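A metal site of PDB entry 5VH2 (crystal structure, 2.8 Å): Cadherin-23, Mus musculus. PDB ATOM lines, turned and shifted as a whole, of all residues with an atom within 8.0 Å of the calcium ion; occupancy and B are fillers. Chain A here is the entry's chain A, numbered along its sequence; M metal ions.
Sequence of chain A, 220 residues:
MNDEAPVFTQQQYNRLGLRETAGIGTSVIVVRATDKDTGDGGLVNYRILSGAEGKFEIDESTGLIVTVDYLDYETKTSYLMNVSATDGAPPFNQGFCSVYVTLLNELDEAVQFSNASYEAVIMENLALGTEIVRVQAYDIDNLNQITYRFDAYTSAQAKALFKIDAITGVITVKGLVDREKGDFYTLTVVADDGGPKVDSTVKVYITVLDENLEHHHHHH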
ATOM      1  N   ASN A   2      -4.344  29.026 -17.098  1.00  0.00           N
ATOM      2  CA  ASN A   2      -4.226  27.536 -17.184  1.00  0.00           C
ATOM      3  C   ASN A   2      -2.800  26.899 -17.109  1.00  0.00           C
ATOM      4  O   ASN A   2      -2.599  25.798 -17.636  1.00  0.00           O
ATOM      5  CB  ASN A   2      -4.983  27.030 -18.443  1.00  0.00           C
ATOM      6  CG  ASN A   2      -4.475  27.644 -19.776  1.00  0.00           C
ATOM      7  OD1 ASN A   2      -3.748  27.002 -20.517  1.00  0.00           O
ATOM      8  ND2 ASN A   2      -4.946  28.836 -20.109  1.00  0.00           N
ATOM      9  N   ASP A   3      -1.817  27.519 -16.436  1.00  0.00           N
ATOM     10  CA  ASP A   3      -0.429  27.062 -16.590  1.00  0.00           C
ATOM     11  C   ASP A   3      -0.305  25.575 -16.218  1.00  0.00           C
ATOM     12  O   ASP A   3       0.290  24.813 -16.981  1.00  0.00           O
ATOM     13  CB  ASP A   3       0.552  28.012 -15.874  1.00  0.00           C
ATOM     14  CG  ASP A   3       2.000  27.452 -15.722  1.00  0.00           C
ATOM     15  OD1 ASP A   3       2.675  27.101 -16.721  1.00  0.00           O
ATOM     16  OD2 ASP A   3       2.512  27.415 -14.560  1.00  0.00           O
ATOM     17  N   GLU A   4      -0.882  25.145 -15.102  1.00  0.00           N
ATOM     18  CA  GLU A   4      -1.155  23.706 -14.864  1.00  0.00           C
ATOM     19  C   GLU A   4      -2.390  23.445 -13.989  1.00  0.00           C
ATOM     20  O   GLU A   4      -2.936  24.338 -13.343  1.00  0.00           O
ATOM     21  CB  GLU A   4       0.064  23.012 -14.232  1.00  0.00           C
ATOM     22  CG  GLU A   4       0.335  23.454 -12.807  1.00  0.00           C
ATOM     23  CD  GLU A   4       1.756  23.308 -12.404  1.00  0.00           C
ATOM     24  OE1 GLU A   4       1.959  22.748 -11.299  1.00  0.00           O
ATOM     25  OE2 GLU A   4       2.642  23.778 -13.167  1.00  0.00           O
ATOM     26  N   ALA A   5      -2.822  22.198 -13.977  1.00  0.00           N
ATOM     27  CA  ALA A   5      -3.974  21.788 -13.196  1.00  0.00           C
ATOM     28  C   ALA A   5      -3.491  21.092 -11.924  1.00  0.00           C
ATOM     29  O   ALA A   5      -2.337  20.651 -11.849  1.00  0.00           O
ATOM     30  CB  ALA A   5      -4.873  20.868 -13.994  1.00  0.00           C
ATOM     31  N   PRO A   6      -4.381  20.983 -10.931  1.00  0.00           N
ATOM     32  CA  PRO A   6      -4.051  20.338  -9.652  1.00  0.00           C
ATOM     33  C   PRO A   6      -3.848  18.840  -9.804  1.00  0.00           C
ATOM     34  O   PRO A   6      -4.584  18.179 -10.542  1.00  0.00           O
ATOM     35  CB  PRO A   6      -5.277  20.604  -8.759  1.00  0.00           C
ATOM     36  CG  PRO A   6      -6.015  21.702  -9.434  1.00  0.00           C
ATOM     37  CD  PRO A   6      -5.772  21.467 -10.918  1.00  0.00           C
ATOM     38  N   THR A  34      -1.830  19.610  -5.200  1.00  0.00           N
ATOM     39  CA  THR A  34      -0.902  20.706  -5.327  1.00  0.00           C
ATOM     40  C   THR A  34      -1.072  21.307  -6.728  1.00  0.00           C
ATOM     41  O   THR A  34      -1.320  20.580  -7.708  1.00  0.00           O
ATOM     42  CB  THR A  34       0.518  20.208  -5.095  1.00  0.00           C
ATOM     43  OG1 THR A  34       0.685  18.973  -5.799  1.00  0.00           O
ATOM     44  CG2 THR A  34       0.707  19.938  -3.649  1.00  0.00           C
ATOM     45  N   ASP A  35      -0.974  22.638  -6.769  1.00  0.00           N
ATOM     46  CA  ASP A  35      -0.982  23.410  -8.006  1.00  0.00           C
ATOM     47  C   ASP A  35       0.103  24.470  -7.838  1.00  0.00           C
ATOM     48  O   ASP A  35       0.131  25.160  -6.838  1.00  0.00           O
ATOM     49  CB  ASP A  35      -2.351  24.035  -8.193  1.00  0.00           C
ATOM     50  CG  ASP A  35      -2.566  24.548  -9.601  1.00  0.00           C
ATOM     51  OD1 ASP A  35      -1.649  25.085 -10.237  1.00  0.00           O
ATOM     52  OD2 ASP A  35      -3.713  24.504 -10.045  1.00  0.00           O
ATOM     53  N   LYS A  36       1.053  24.501  -8.765  1.00  0.00           N
ATOM     54  CA  LYS A  36       2.271  25.310  -8.570  1.00  0.00           C
ATOM     55  C   LYS A  36       2.234  26.587  -9.409  1.00  0.00           C
ATOM     56  O   LYS A  36       3.197  27.327  -9.436  1.00  0.00           O
ATOM     57  CB  LYS A  36       3.535  24.502  -8.844  1.00  0.00           C
ATOM     58  CG  LYS A  36       3.612  23.210  -7.989  1.00  0.00           C
ATOM     59  CD  LYS A  36       4.868  22.372  -8.091  1.00  0.00           C
ATOM     60  CE  LYS A  36       5.495  22.343  -9.476  1.00  0.00           C
ATOM     61  NZ  LYS A  36       4.596  21.902 -10.581  1.00  0.00           N
ATOM     62  N   ASP A  37       1.075  26.883  -9.991  1.00  0.00           N
ATOM     63  CA  ASP A  37       0.739  28.248 -10.399  1.00  0.00           C
ATOM     64  C   ASP A  37       0.685  29.139  -9.195  1.00  0.00           C
ATOM     65  O   ASP A  37       0.252  28.700  -8.134  1.00  0.00           O
ATOM     66  CB  ASP A  37      -0.643  28.291 -11.041  1.00  0.00           C
ATOM     67  CG  ASP A  37      -0.729  27.426 -12.280  1.00  0.00           C
ATOM     68  OD1 ASP A  37       0.331  27.063 -12.795  1.00  0.00           O
ATOM     69  OD2 ASP A  37      -1.838  27.030 -12.709  1.00  0.00           O
ATOM     70  N   THR A  38       1.115  30.385  -9.359  1.00  0.00           N
ATOM     71  CA  THR A  38       0.971  31.410  -8.308  1.00  0.00           C
ATOM     72  C   THR A  38      -0.456  31.886  -8.180  1.00  0.00           C
ATOM     73  O   THR A  38      -1.309  31.621  -9.025  1.00  0.00           O
ATOM     74  CB  THR A  38       1.821  32.652  -8.614  1.00  0.00           C
ATOM     75  OG1 THR A  38       1.493  33.115  -9.927  1.00  0.00           O
ATOM     76  CG2 THR A  38       3.299  32.331  -8.533  1.00  0.00           C
ATOM     77  N   GLY A  39      -0.695  32.607  -7.098  1.00  0.00           N
ATOM     78  CA  GLY A  39      -1.950  33.339  -6.900  1.00  0.00           C
ATOM     79  C   GLY A  39      -3.128  32.406  -6.972  1.00  0.00           C
ATOM     80  O   GLY A  39      -2.993  31.266  -6.594  1.00  0.00           O
ATOM     81  N   ASP A  40      -4.235  32.840  -7.538  1.00  0.00           N
ATOM     82  CA  ASP A  40      -5.475  32.032  -7.504  1.00  0.00           C
ATOM     83  C   ASP A  40      -5.448  30.812  -8.425  1.00  0.00           C
ATOM     84  O   ASP A  40      -6.167  29.833  -8.199  1.00  0.00           O
ATOM     85  CB  ASP A  40      -6.685  32.876  -7.898  1.00  0.00           C
ATOM     86  CG  ASP A  40      -6.919  34.006  -6.958  1.00  0.00           C
ATOM     87  OD1 ASP A  40      -6.552  33.833  -5.760  1.00  0.00           O
ATOM     88  OD2 ASP A  40      -7.483  35.040  -7.448  1.00  0.00           O
ATOM     89  N   GLY A  41      -4.585  30.860  -9.433  1.00  0.00           N
ATOM     90  CA  GLY A  41      -4.324  29.723 -10.300  1.00  0.00           C
ATOM     91  C   GLY A  41      -3.731  28.520  -9.610  1.00  0.00           C
ATOM     92  O   GLY A  41      -3.841  27.408 -10.140  1.00  0.00           O
ATOM     93  N   GLY A  42      -3.174  28.712  -8.414  1.00  0.00           N
ATOM     94  CA  GLY A  42      -2.594  27.636  -7.615  1.00  0.00           C
ATOM     95  C   GLY A  42      -3.376  27.308  -6.342  1.00  0.00           C
ATOM     96  O   GLY A  42      -2.899  26.585  -5.495  1.00  0.00           O
ATOM     97  N   LEU A  43      -4.586  27.853  -6.233  1.00  0.00           N
ATOM     98  CA  LEU A  43      -5.422  27.700  -5.051  1.00  0.00           C
ATOM     99  C   LEU A  43      -6.596  26.794  -5.416  1.00  0.00           C
ATOM    100  O   LEU A  43      -7.455  27.132  -6.222  1.00  0.00           O
ATOM    101  CB  LEU A  43      -5.952  29.063  -4.639  1.00  0.00           C
ATOM    102  CG  LEU A  43      -6.690  29.359  -3.339  1.00  0.00           C
ATOM    103  CD1 LEU A  43      -6.260  30.773  -2.921  1.00  0.00           C
ATOM    104  CD2 LEU A  43      -8.230  29.290  -3.360  1.00  0.00           C
ATOM    105  N   VAL A  44      -6.677  25.647  -4.754  1.00  0.00           N
ATOM    106  CA  VAL A  44      -7.590  24.630  -5.170  1.00  0.00           C
ATOM    107  C   VAL A  44      -8.785  24.496  -4.251  1.00  0.00           C
ATOM    108  O   VAL A  44      -8.641  24.715  -3.045  1.00  0.00           O
ATOM    109  CB  VAL A  44      -6.868  23.310  -5.286  1.00  0.00           C
ATOM    110  CG1 VAL A  44      -5.512  23.524  -5.927  1.00  0.00           C
ATOM    111  CG2 VAL A  44      -6.732  22.641  -3.936  1.00  0.00           C
ATOM    112  N   THR A  86     -10.381  21.840  -8.025  1.00  0.00           N
ATOM    113  CA  THR A  86     -10.531  22.828  -9.076  1.00  0.00           C
ATOM    114  C   THR A  86      -9.665  24.024  -8.706  1.00  0.00           C
ATOM    115  O   THR A  86      -9.793  24.537  -7.600  1.00  0.00           O
ATOM    116  CB  THR A  86     -11.995  23.232  -9.121  1.00  0.00           C
ATOM    117  OG1 THR A  86     -12.792  22.069  -9.324  1.00  0.00           O
ATOM    118  CG2 THR A  86     -12.261  24.176 -10.217  1.00  0.00           C
ATOM    119  N   ASP A  87      -8.752  24.470  -9.565  1.00  0.00           N
ATOM    120  CA  ASP A  87      -8.005  25.701  -9.248  1.00  0.00           C
ATOM    121  C   ASP A  87      -8.896  26.961  -9.304  1.00  0.00           C
ATOM    122  O   ASP A  87     -10.030  26.905  -9.796  1.00  0.00           O
ATOM    123  CB  ASP A  87      -6.680  25.866 -10.009  1.00  0.00           C
ATOM    124  CG  ASP A  87      -6.841  26.023 -11.491  1.00  0.00           C
ATOM    125  OD1 ASP A  87      -7.978  26.158 -11.945  1.00  0.00           O
ATOM    126  OD2 ASP A  87      -5.778  25.976 -12.186  1.00  0.00           O
ATOM    127  N   GLY A  88      -8.417  28.035  -8.692  1.00  0.00           N
ATOM    128  CA  GLY A  88      -9.256  29.147  -8.233  1.00  0.00           C
ATOM    129  C   GLY A  88      -9.386  30.265  -9.229  1.00  0.00           C
ATOM    130  O   GLY A  88     -10.009  31.251  -8.948  1.00  0.00           O
ATOM    131  N   ALA A  89      -8.793  30.100 -10.401  1.00  0.00           N
ATOM    132  CA  ALA A  89      -8.893  31.091 -11.451  1.00  0.00           C
ATOM    133  C   ALA A  89      -9.379  30.401 -12.715  1.00  0.00           C
ATOM    134  O   ALA A  89      -9.172  29.203 -12.881  1.00  0.00           O
ATOM    135  CB  ALA A  89      -7.543  31.735 -11.692  1.00  0.00           C
ATOM    136  N   PRO A  90      -9.975  31.171 -13.644  1.00  0.00           N
ATOM    137  CA  PRO A  90     -10.197  30.708 -15.010  1.00  0.00           C
ATOM    138  C   PRO A  90      -8.954  30.018 -15.593  1.00  0.00           C
ATOM    139  O   PRO A  90      -7.848  30.536 -15.428  1.00  0.00           O
ATOM    140  CB  PRO A  90     -10.461  32.019 -15.765  1.00  0.00           C
ATOM    141  CG  PRO A  90     -11.115  32.893 -14.761  1.00  0.00           C
ATOM    142  CD  PRO A  90     -10.563  32.501 -13.422  1.00  0.00           C
ATOM    143  N   PRO A  91      -9.114  28.884 -16.287  1.00  0.00           N
ATOM    144  CA  PRO A  91     -10.414  28.264 -16.632  1.00  0.00           C
ATOM    145  C   PRO A  91     -10.897  27.175 -15.642  1.00  0.00           C
ATOM    146  O   PRO A  91     -11.638  26.285 -16.042  1.00  0.00           O
ATOM    147  CB  PRO A  91     -10.117  27.640 -17.986  1.00  0.00           C
ATOM    148  CG  PRO A  91      -8.676  27.260 -17.899  1.00  0.00           C
ATOM    149  CD  PRO A  91      -8.017  28.350 -17.112  1.00  0.00           C
ATOM    150  N   PHE A  92     -10.466  27.247 -14.392  1.00  0.00           N
ATOM    151  CA  PHE A  92     -10.901  26.326 -13.351  1.00  0.00           C
ATOM    152  C   PHE A  92     -10.513  24.894 -13.676  1.00  0.00           C
ATOM    153  O   PHE A  92     -11.362  23.998 -13.723  1.00  0.00           O
ATOM    154  CB  PHE A  92     -12.417  26.469 -13.095  1.00  0.00           C
ATOM    155  CG  PHE A  92     -12.841  27.885 -12.842  1.00  0.00           C
ATOM    156  CD1 PHE A  92     -12.388  28.548 -11.699  1.00  0.00           C
ATOM    157  CD2 PHE A  92     -13.624  28.579 -13.755  1.00  0.00           C
ATOM    158  CE1 PHE A  92     -12.725  29.856 -11.458  1.00  0.00           C
ATOM    159  CE2 PHE A  92     -13.973  29.909 -13.515  1.00  0.00           C
ATOM    160  CZ  PHE A  92     -13.539  30.537 -12.344  1.00  0.00           C
ATOM    161  N   ASN A  93      -9.216  24.680 -13.881  1.00  0.00           N
ATOM    162  CA  ASN A  93      -8.728  23.364 -14.307  1.00  0.00           C
ATOM    163  C   ASN A  93      -8.976  22.410 -13.154  1.00  0.00           C
ATOM    164  O   ASN A  93      -8.819  22.807 -12.003  1.00  0.00           O
ATOM    165  CB  ASN A  93      -7.220  23.402 -14.605  1.00  0.00           C
ATOM    166  CG  ASN A  93      -6.852  24.449 -15.649  1.00  0.00           C
ATOM    167  OD1 ASN A  93      -7.121  24.300 -16.840  1.00  0.00           O
ATOM    168  ND2 ASN A  93      -6.203  25.508 -15.202  1.00  0.00           N
ATOM    169  N   GLN A  94      -9.331  21.161 -13.457  1.00  0.00           N
ATOM    170  CA  GLN A  94      -9.641  20.186 -12.445  1.00  0.00           C
ATOM    171  C   GLN A  94      -8.590  19.088 -12.381  1.00  0.00           C
ATOM    172  O   GLN A  94      -7.936  18.757 -13.383  1.00  0.00           O
ATOM    173  CB  GLN A  94     -10.984  19.545 -12.725  1.00  0.00           C
ATOM    174  CG  GLN A  94     -12.173  20.422 -12.419  1.00  0.00           C
ATOM    175  CD  GLN A  94     -13.462  19.725 -12.916  1.00  0.00           C
ATOM    176  OE1 GLN A  94     -14.198  19.088 -12.165  1.00  0.00           O
ATOM    177  NE2 GLN A  94     -13.710  19.843 -14.221  1.00  0.00           N
HETATM  178 CA    CA M   1      -3.682  26.172 -12.389  1.00  0.00          CA
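OE1 of Glu 4 lies within salt-bridge range of NZ of Lys 36 (2.9 Å).
The backbone NH of Gly 42 sits close to the backbone carbonyl oxygen of Asp 37 (3.4 Å).
OD1 of Asp 87 sits at hydrogen-bond distance from N of Asn 93.
Residues that only touch the calcium ion: Asn 93.
Six residues have an atom within 4 Å of the calcium ion: Glu 4, Asp 35, Asp 37, Gly 41, Asp 87 and Asn 93.
The calcium ion is bound by the side-chain carboxylate (OD2) of Asp 37 (2.1 Å), the side-chain carboxylate (OD2) of Asp 87 (2.1 Å), the backbone carbonyl oxygen (O) of Glu 4 (2.2 Å), the backbone carbonyl oxygen (O) of Gly 41 (2.6 Å) and the side-chain carboxylate (OD2) of Asp 35 (2.9 Å).
The calcium ion has five donor atoms within binding distance.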
